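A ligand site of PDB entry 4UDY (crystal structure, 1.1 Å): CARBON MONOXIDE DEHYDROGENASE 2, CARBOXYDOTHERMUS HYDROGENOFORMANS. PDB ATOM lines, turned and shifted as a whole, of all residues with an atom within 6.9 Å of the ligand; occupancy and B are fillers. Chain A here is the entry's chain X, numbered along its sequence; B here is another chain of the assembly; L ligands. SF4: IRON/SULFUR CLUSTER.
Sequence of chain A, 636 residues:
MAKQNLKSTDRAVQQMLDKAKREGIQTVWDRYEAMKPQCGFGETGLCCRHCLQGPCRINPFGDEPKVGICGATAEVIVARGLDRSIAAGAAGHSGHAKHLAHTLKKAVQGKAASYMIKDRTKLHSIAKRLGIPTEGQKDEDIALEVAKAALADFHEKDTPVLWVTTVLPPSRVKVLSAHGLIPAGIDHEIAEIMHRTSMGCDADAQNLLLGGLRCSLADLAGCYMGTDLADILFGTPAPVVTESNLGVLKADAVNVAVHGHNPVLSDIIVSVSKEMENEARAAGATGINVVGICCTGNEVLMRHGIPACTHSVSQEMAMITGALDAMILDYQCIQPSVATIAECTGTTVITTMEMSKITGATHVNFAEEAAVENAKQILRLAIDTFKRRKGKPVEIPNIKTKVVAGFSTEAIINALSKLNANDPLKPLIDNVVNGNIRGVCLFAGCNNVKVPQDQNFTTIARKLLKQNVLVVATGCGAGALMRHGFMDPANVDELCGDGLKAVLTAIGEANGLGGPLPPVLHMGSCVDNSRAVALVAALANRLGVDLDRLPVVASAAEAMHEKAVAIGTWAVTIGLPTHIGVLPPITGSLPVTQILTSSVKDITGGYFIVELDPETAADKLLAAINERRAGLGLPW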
ATOM      1  N   CYS A  47       9.263 -11.814   2.921  1.00  0.00           N
ATOM      2  CA  CYS A  47      10.225 -11.982   3.996  1.00  0.00           C
ATOM      3  C   CYS A  47      11.590 -12.224   3.347  1.00  0.00           C
ATOM      4  O   CYS A  47      11.668 -12.948   2.320  1.00  0.00           O
ATOM      5  CB  CYS A  47       9.871 -13.123   4.951  1.00  0.00           C
ATOM      6  SG  CYS A  47      11.139 -13.369   6.232  1.00  0.00           S
ATOM      7  N   CYS A  48      12.613 -11.616   3.907  1.00  0.00           N
ATOM      8  CA  CYS A  48      13.979 -11.783   3.465  1.00  0.00           C
ATOM      9  C   CYS A  48      14.903 -11.960   4.674  1.00  0.00           C
ATOM     10  O   CYS A  48      14.852 -11.173   5.604  1.00  0.00           O
ATOM     11  CB  CYS A  48      14.435 -10.584   2.632  1.00  0.00           C
ATOM     12  SG  CYS A  48      16.127 -10.739   1.986  1.00  0.00           S
ATOM     13  N   ARG A  49      15.775 -12.978   4.567  1.00  0.00           N
ATOM     14  CA  ARG A  49      16.806 -13.281   5.522  1.00  0.00           C
ATOM     15  C   ARG A  49      18.170 -13.381   4.844  1.00  0.00           C
ATOM     16  O   ARG A  49      19.045 -14.128   5.287  1.00  0.00           O
ATOM     17  CB  ARG A  49      16.481 -14.543   6.325  1.00  0.00           C
ATOM     18  CG  ARG A  49      15.228 -14.406   7.131  1.00  0.00           C
ATOM     19  CD  ARG A  49      14.757 -15.755   7.660  1.00  0.00           C
ATOM     20  NE  ARG A  49      15.750 -16.365   8.461  1.00  0.00           N
ATOM     21  CZ  ARG A  49      15.916 -17.625   8.775  1.00  0.00           C
ATOM     22  NH1 ARG A  49      15.009 -18.506   8.342  1.00  0.00           N
ATOM     23  NH2 ARG A  49      16.946 -17.967   9.536  1.00  0.00           N
ATOM     24  N   HIS A  50      18.354 -12.641   3.738  1.00  0.00           N
ATOM     25  CA  HIS A  50      19.594 -12.729   2.985  1.00  0.00           C
ATOM     26  C   HIS A  50      20.762 -11.995   3.599  1.00  0.00           C
ATOM     27  O   HIS A  50      21.857 -12.097   3.056  1.00  0.00           O
ATOM     28  CB  HIS A  50      19.397 -12.369   1.515  1.00  0.00           C
ATOM     29  CG  HIS A  50      18.491 -13.306   0.789  1.00  0.00           C
ATOM     30  ND1 HIS A  50      18.430 -13.328  -0.584  1.00  0.00           N
ATOM     31  CD2 HIS A  50      17.603 -14.241   1.188  1.00  0.00           C
ATOM     32  CE1 HIS A  50      17.521 -14.236  -0.959  1.00  0.00           C
ATOM     33  NE2 HIS A  50      16.997 -14.831   0.084  1.00  0.00           N
ATOM     34  N   CYS A  51      20.610 -11.287   4.697  1.00  0.00           N
ATOM     35  CA  CYS A  51      21.765 -10.765   5.424  1.00  0.00           C
ATOM     36  C   CYS A  51      21.427 -10.655   6.904  1.00  0.00           C
ATOM     37  O   CYS A  51      20.290 -10.844   7.311  1.00  0.00           O
ATOM     38  CB  CYS A  51      22.297  -9.440   4.864  1.00  0.00           C
ATOM     39  SG  CYS A  51      21.357  -7.961   5.365  1.00  0.00           S
ATOM     40  N   LEU A  52      22.453 -10.320   7.688  1.00  0.00           N
ATOM     41  CA  LEU A  52      22.305 -10.273   9.153  1.00  0.00           C
ATOM     42  C   LEU A  52      21.708  -8.970   9.643  1.00  0.00           C
ATOM     43  O   LEU A  52      21.601  -8.804  10.872  1.00  0.00           O
ATOM     44  CB  LEU A  52      23.665 -10.566   9.816  1.00  0.00           C
ATOM     45  CG  LEU A  52      24.297 -11.899   9.487  1.00  0.00           C
ATOM     46  CD1 LEU A  52      25.613 -11.971  10.218  1.00  0.00           C
ATOM     47  CD2 LEU A  52      23.375 -13.045   9.822  1.00  0.00           C
ATOM     48  N   GLN A  53      21.307  -8.049   8.740  1.00  0.00           N
ATOM     49  CA  GLN A  53      20.447  -6.976   9.154  1.00  0.00           C
ATOM     50  C   GLN A  53      19.003  -7.440   9.263  1.00  0.00           C
ATOM     51  O   GLN A  53      18.216  -6.769   9.919  1.00  0.00           O
ATOM     52  CB  GLN A  53      20.501  -5.780   8.196  1.00  0.00           C
ATOM     53  CG  GLN A  53      21.858  -5.130   8.267  1.00  0.00           C
ATOM     54  CD  GLN A  53      22.079  -3.990   7.343  1.00  0.00           C
ATOM     55  OE1 GLN A  53      21.446  -3.877   6.256  1.00  0.00           O
ATOM     56  NE2 GLN A  53      22.936  -3.138   7.617  1.00  0.00           N
ATOM     57  N   GLY A  54      18.653  -8.559   8.628  1.00  0.00           N
ATOM     58  CA  GLY A  54      17.350  -9.104   8.727  1.00  0.00           C
ATOM     59  C   GLY A  54      17.054  -9.784  10.037  1.00  0.00           C
ATOM     60  O   GLY A  54      17.889  -9.755  10.968  1.00  0.00           O
ATOM     61  N   PRO A  55      15.901 -10.419  10.186  1.00  0.00           N
ATOM     62  CA  PRO A  55      14.924 -10.642   9.103  1.00  0.00           C
ATOM     63  C   PRO A  55      14.148  -9.381   8.767  1.00  0.00           C
ATOM     64  O   PRO A  55      13.807  -8.569   9.629  1.00  0.00           O
ATOM     65  CB  PRO A  55      14.025 -11.695   9.736  1.00  0.00           C
ATOM     66  CG  PRO A  55      14.095 -11.432  11.223  1.00  0.00           C
ATOM     67  CD  PRO A  55      15.512 -11.044  11.448  1.00  0.00           C
ATOM     68  N   CYS A  56      13.924  -9.216   7.464  1.00  0.00           N
ATOM     69  CA  CYS A  56      13.099  -8.161   6.941  1.00  0.00           C
ATOM     70  C   CYS A  56      11.797  -8.728   6.468  1.00  0.00           C
ATOM     71  O   CYS A  56      11.722  -9.857   5.986  1.00  0.00           O
ATOM     72  CB  CYS A  56      13.767  -7.420   5.785  1.00  0.00           C
ATOM     73  SG  CYS A  56      15.220  -6.426   6.328  1.00  0.00           S
ATOM     74  N   ARG A  57      10.740  -7.964   6.563  1.00  0.00           N
ATOM     75  CA  ARG A  57       9.411  -8.291   6.044  1.00  0.00           C
ATOM     76  C   ARG A  57       8.790  -7.032   5.487  1.00  0.00           C
ATOM     77  O   ARG A  57       9.193  -5.912   5.808  1.00  0.00           O
ATOM     78  CB  ARG A  57       8.543  -8.912   7.142  1.00  0.00           C
ATOM     79  CG  ARG A  57       8.094  -7.938   8.190  1.00  0.00           C
ATOM     80  CD  ARG A  57       7.677  -8.571   9.519  1.00  0.00           C
ATOM     81  NE  ARG A  57       7.164  -7.482  10.378  1.00  0.00           N
ATOM     82  CZ  ARG A  57       7.962  -6.619  11.000  1.00  0.00           C
ATOM     83  NH1 ARG A  57       9.289  -6.732  11.012  1.00  0.00           N
ATOM     84  NH2 ARG A  57       7.398  -5.622  11.700  1.00  0.00           N
ATOM     85  N   VAL A  67       9.392  -1.716   2.821  1.00  0.00           N
ATOM     86  CA  VAL A  67      10.625  -1.949   2.076  1.00  0.00           C
ATOM     87  C   VAL A  67      11.636  -2.610   2.985  1.00  0.00           C
ATOM     88  O   VAL A  67      11.599  -2.366   4.215  1.00  0.00           O
ATOM     89  CB  VAL A  67      11.108  -0.592   1.509  1.00  0.00           C
ATOM     90  CG1 VAL A  67      11.380   0.396   2.624  1.00  0.00           C
ATOM     91  CG2 VAL A  67      12.244  -0.749   0.592  1.00  0.00           C
ATOM     92  N   GLY A  68      12.512  -3.403   2.439  1.00  0.00           N
ATOM     93  CA  GLY A  68      13.585  -3.982   3.232  1.00  0.00           C
ATOM     94  C   GLY A  68      14.555  -2.951   3.728  1.00  0.00           C
ATOM     95  O   GLY A  68      14.644  -1.846   3.238  1.00  0.00           O
ATOM     96  N   ILE A  69      15.359  -3.335   4.721  1.00  0.00           N
ATOM     97  CA  ILE A  69      16.282  -2.411   5.334  1.00  0.00           C
ATOM     98  C   ILE A  69      17.284  -1.822   4.329  1.00  0.00           C
ATOM     99  O   ILE A  69      17.586  -0.633   4.370  1.00  0.00           O
ATOM    100  CB  ILE A  69      16.960  -3.031   6.565  1.00  0.00           C
ATOM    101  CG1 ILE A  69      15.968  -3.192   7.707  1.00  0.00           C
ATOM    102  CG2 ILE A  69      18.182  -2.230   7.000  1.00  0.00           C
ATOM    103  CD1 ILE A  69      16.430  -4.051   8.871  1.00  0.00           C
ATOM    104  N   CYS A  70      17.791  -2.675   3.432  1.00  0.00           N
ATOM    105  CA  CYS A  70      18.738  -2.197   2.399  1.00  0.00           C
ATOM    106  C   CYS A  70      18.087  -1.452   1.267  1.00  0.00           C
ATOM    107  O   CYS A  70      18.806  -0.954   0.370  1.00  0.00           O
ATOM    108  CB  CYS A  70      19.482  -3.418   1.834  1.00  0.00           C
ATOM    109  SG  CYS A  70      18.359  -4.579   1.015  1.00  0.00           S
ATOM    110  N   GLY A  71      16.757  -1.376   1.272  1.00  0.00           N
ATOM    111  CA  GLY A  71      15.993  -0.784   0.180  1.00  0.00           C
ATOM    112  C   GLY A  71      15.374  -1.787  -0.766  1.00  0.00           C
ATOM    113  O   GLY A  71      14.750  -1.406  -1.754  1.00  0.00           O
ATOM    114  N   ALA A  72      15.511  -3.086  -0.507  1.00  0.00           N
ATOM    115  CA  ALA A  72      14.933  -4.109  -1.368  1.00  0.00           C
ATOM    116  C   ALA A  72      13.403  -3.958  -1.350  1.00  0.00           C
ATOM    117  O   ALA A  72      12.769  -4.013  -0.306  1.00  0.00           O
ATOM    118  CB  ALA A  72      15.376  -5.496  -0.944  1.00  0.00           C
ATOM    119  N   THR A  73      12.826  -3.848  -2.561  1.00  0.00           N
ATOM    120  CA  THR A  73      11.386  -3.746  -2.686  1.00  0.00           C
ATOM    121  C   THR A  73      10.723  -5.104  -2.583  1.00  0.00           C
ATOM    122  O   THR A  73      11.356  -6.165  -2.640  1.00  0.00           O
ATOM    123  CB  THR A  73      11.038  -3.116  -4.041  1.00  0.00           C
ATOM    124  OG1 THR A  73      11.532  -4.012  -5.036  1.00  0.00           O
ATOM    125  CG2 THR A  73      11.618  -1.727  -4.230  1.00  0.00           C
ATOM    126  N   ILE A  77      12.439  -8.773  -3.334  1.00  0.00           N
ATOM    127  CA  ILE A  77      12.450  -9.806  -2.302  1.00  0.00           C
ATOM    128  C   ILE A  77      11.732 -11.069  -2.830  1.00  0.00           C
ATOM    129  O   ILE A  77      12.249 -12.184  -2.718  1.00  0.00           O
ATOM    130  CB  ILE A  77      11.834  -9.285  -0.990  1.00  0.00           C
ATOM    131  CG1 ILE A  77      12.795  -8.285  -0.332  1.00  0.00           C
ATOM    132  CG2 ILE A  77      11.400 -10.411  -0.096  1.00  0.00           C
ATOM    133  CD1 ILE A  77      12.204  -7.600   0.858  1.00  0.00           C
ATOM    134  N   ARG A  80      13.869 -12.732  -5.599  1.00  0.00           N
ATOM    135  CA  ARG A  80      15.071 -13.374  -5.085  1.00  0.00           C
ATOM    136  C   ARG A  80      14.754 -14.690  -4.399  1.00  0.00           C
ATOM    137  O   ARG A  80      15.479 -15.687  -4.532  1.00  0.00           O
ATOM    138  CB  ARG A  80      15.817 -12.420  -4.120  1.00  0.00           C
ATOM    139  CG  ARG A  80      16.406 -11.187  -4.817  1.00  0.00           C
ATOM    140  CD  ARG A  80      17.389 -10.395  -3.997  1.00  0.00           C
ATOM    141  NE  ARG A  80      16.842 -10.008  -2.680  1.00  0.00           N
ATOM    142  CZ  ARG A  80      17.409  -9.106  -1.890  1.00  0.00           C
ATOM    143  NH1 ARG A  80      18.501  -8.492  -2.259  1.00  0.00           N
ATOM    144  NH2 ARG A  80      16.868  -8.811  -0.717  1.00  0.00           N
ATOM    145  N   THR A 197      21.262 -13.065  -6.026  1.00  0.00           N
ATOM    146  CA  THR A 197      20.223 -12.914  -5.036  1.00  0.00           C
ATOM    147  C   THR A 197      20.754 -12.571  -3.649  1.00  0.00           C
ATOM    148  O   THR A 197      19.929 -12.305  -2.743  1.00  0.00           O
ATOM    149  CB  THR A 197      19.336 -14.174  -4.942  1.00  0.00           C
ATOM    150  OG1 THR A 197      20.167 -15.275  -4.633  1.00  0.00           O
ATOM    151  CG2 THR A 197      18.576 -14.472  -6.221  1.00  0.00           C
ATOM    152  N   SER A 198      22.073 -12.563  -3.464  1.00  0.00           N
ATOM    153  CA  SER A 198      22.674 -12.115  -2.214  1.00  0.00           C
ATOM    154  C   SER A 198      22.516 -10.609  -2.067  1.00  0.00           C
ATOM    155  O   SER A 198      22.157  -9.907  -2.994  1.00  0.00           O
ATOM    156  CB  SER A 198      24.097 -12.622  -2.110  1.00  0.00           C
ATOM    157  OG  SER A 198      25.023 -11.912  -2.889  1.00  0.00           O
ATOM    158  N   MET A 199      22.775 -10.134  -0.848  1.00  0.00           N
ATOM    159  CA  MET A 199      22.497  -8.734  -0.569  1.00  0.00           C
ATOM    160  C   MET A 199      23.314  -7.808  -1.483  1.00  0.00           C
ATOM    161  O   MET A 199      24.488  -7.981  -1.768  1.00  0.00           O
ATOM    162  CB  MET A 199      22.740  -8.452   0.917  1.00  0.00           C
ATOM    163  CG  MET A 199      22.471  -7.016   1.340  1.00  0.00           C
ATOM    164  SD  MET A 199      23.880  -5.931   1.006  1.00  0.00           S
ATOM    165  CE  MET A 199      23.110  -4.354   0.910  1.00  0.00           C
ATOM    166  N   GLY A 200      22.610  -6.786  -1.970  1.00  0.00           N
ATOM    167  CA  GLY A 200      23.266  -5.739  -2.700  1.00  0.00           C
ATOM    168  C   GLY A 200      23.734  -6.073  -4.096  1.00  0.00           C
ATOM    169  O   GLY A 200      24.654  -5.423  -4.618  1.00  0.00           O
ATOM    170  N   VAL B  28      18.839   4.040   5.394  1.00  0.00           N
ATOM    171  CA  VAL B  28      18.892   2.694   5.958  1.00  0.00           C
ATOM    172  C   VAL B  28      18.504   2.680   7.405  1.00  0.00           C
ATOM    173  O   VAL B  28      17.836   1.737   7.868  1.00  0.00           O
ATOM    174  CB  VAL B  28      20.292   2.111   5.710  1.00  0.00           C
ATOM    175  CG1 VAL B  28      21.398   2.915   6.453  1.00  0.00           C
ATOM    176  CG2 VAL B  28      20.337   0.654   6.048  1.00  0.00           C
ATOM    177  N   MET B  35      11.232  -1.348  10.580  1.00  0.00           N
ATOM    178  CA  MET B  35      11.177  -2.796  10.610  1.00  0.00           C
ATOM    179  C   MET B  35      11.006  -3.332  12.021  1.00  0.00           C
ATOM    180  O   MET B  35      10.729  -4.526  12.192  1.00  0.00           O
ATOM    181  CB  MET B  35      12.478  -3.356   9.985  1.00  0.00           C
ATOM    182  CG  MET B  35      12.387  -4.812   9.536  1.00  0.00           C
ATOM    183  SD  MET B  35      11.134  -5.068   8.260  1.00  0.00           S
ATOM    184  CE  MET B  35      11.861  -4.223   6.865  1.00  0.00           C
ATOM    185  N   GLN B  38      11.716  -6.757  14.856  1.00  0.00           N
ATOM    186  CA  GLN B  38      11.955  -7.802  13.859  1.00  0.00           C
ATOM    187  C   GLN B  38      11.436  -9.152  14.336  1.00  0.00           C
ATOM    188  O   GLN B  38      11.308  -9.407  15.521  1.00  0.00           O
ATOM    189  CB  GLN B  38      13.422  -7.811  13.469  1.00  0.00           C
ATOM    190  CG  GLN B  38      13.847  -6.538  12.764  1.00  0.00           C
ATOM    191  CD  GLN B  38      15.312  -6.521  12.390  1.00  0.00           C
ATOM    192  OE1 GLN B  38      16.162  -6.214  13.220  1.00  0.00           O
ATOM    193  NE2 GLN B  38      15.615  -6.849  11.142  1.00  0.00           N
ATOM    194  N   PRO B 336      20.082  -1.147  -2.671  1.00  0.00           N
ATOM    195  CA  PRO B 336      19.338  -0.734  -3.863  1.00  0.00           C
ATOM    196  C   PRO B 336      18.601   0.584  -3.696  1.00  0.00           C
ATOM    197  O   PRO B 336      18.176   1.184  -4.670  1.00  0.00           O
ATOM    198  CB  PRO B 336      18.458  -1.929  -4.165  1.00  0.00           C
ATOM    199  CG  PRO B 336      18.275  -2.622  -2.838  1.00  0.00           C
ATOM    200  CD  PRO B 336      19.625  -2.475  -2.170  1.00  0.00           C
ATOM    201  N   MET B 560      27.476  -8.345   8.356  1.00  0.00           N
ATOM    202  CA  MET B 560      26.195  -8.209   7.659  1.00  0.00           C
ATOM    203  C   MET B 560      26.003  -9.254   6.564  1.00  0.00           C
ATOM    204  O   MET B 560      25.004  -9.977   6.566  1.00  0.00           O
ATOM    205  CB  MET B 560      26.057  -6.760   7.120  1.00  0.00           C
ATOM    206  CG  MET B 560      24.779  -6.456   6.336  1.00  0.00           C
ATOM    207  SD  MET B 560      24.856  -6.766   4.567  1.00  0.00           S
ATOM    208  CE  MET B 560      26.175  -5.664   4.084  1.00  0.00           C
HETATM  209 FE1  SF4 L   1      16.832  -7.087   4.805  1.00  0.00          FE
HETATM  210 FE2  SF4 L   1      19.341  -7.986   4.310  1.00  0.00          FE
HETATM  211 FE3  SF4 L   1      17.220  -8.936   2.910  1.00  0.00          FE
HETATM  212 FE4  SF4 L   1      18.039  -6.381   2.447  1.00  0.00          FE
HETATM  213  S1  SF4 L   1      19.200  -8.348   2.003  1.00  0.00           S
HETATM  214  S2  SF4 L   1      15.877  -7.047   2.668  1.00  0.00           S
HETATM  215  S3  SF4 L   1      18.655  -5.769   4.625  1.00  0.00           S
HETATM  216  S4  SF4 L   1      17.638  -9.243   5.167  1.00  0.00           S
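The backbone carbonyl oxygen (O) of Cys 48 is in hydrogen-bond range of the backbone NH (N) of Cys 56 (2.9 Å).
A ring nitrogen (ND1) of His 50 lies within hydrogen-bond range of the backbone carbonyl oxygen (O) of Thr 197 (2.8 Å).
The backbone carbonyl oxygen (O) of Gln 53 is in hydrogen-bond range of the side-chain amide nitrogen (NE2) of Gln 38 of chain B, 2.9 Å away.
The backbone carbonyl oxygen (O) of Cys 56 sits close to the side-chain sulfur (SG) of Cys 47, 3.6 Å away.
SG of Cys 48 sits close to NH2 of Arg 80 (3.4 Å).
The backbone NH (N) of Ile 69 sits close to the side-chain sulfur (SG) of Cys 56.
The side-chain sulfur (SG) of Cys 51 lies close to the side-chain sulfur (SD) of Met 560 of chain B, at 3.8 Å.
The side-chain sulfur of Cys 51 lies close to the backbone NH of Gln 53 (3.4 Å).
Merely in contact with the ligand: Gly 68 (3.9 Å), Ile 69 (3.8 Å), Ala 72 (3.96 Å) and Met 199 (3.6 Å).
The nearest printed residue that does not touch the ligand is Ile 77 (4.1 Å).
SG of Cys 56 is bound to FE1 of the ligand.
N of Cys 51 sits close to S4 of the ligand (3.6 Å).
The side-chain sulfur (SG) of Cys 51 is bound to an iron atom (FE2) of the ligand, 2.3 Å away.
FE4 of the ligand is bound by SG of Cys 70.
S3 of the ligand sits close to N of Cys 70, at 3.4 Å.
N of His 50 lies close to S4 of the ligand, 3.8 Å away.
A sulfur (S1) of the ligand sits close to the guanidinium group of Arg 80, at 3.6 Å.
FE3 of the ligand is bound by SG of Cys 48, at 2.3 Å.
The side-chain amide oxygen of Gln 53 lies close to a sulfur (S3) of the ligand (3.7 Å).
The backbone NH (N) of Gly 54 lies close to a sulfur (S4) of the ligand (3.7 Å).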
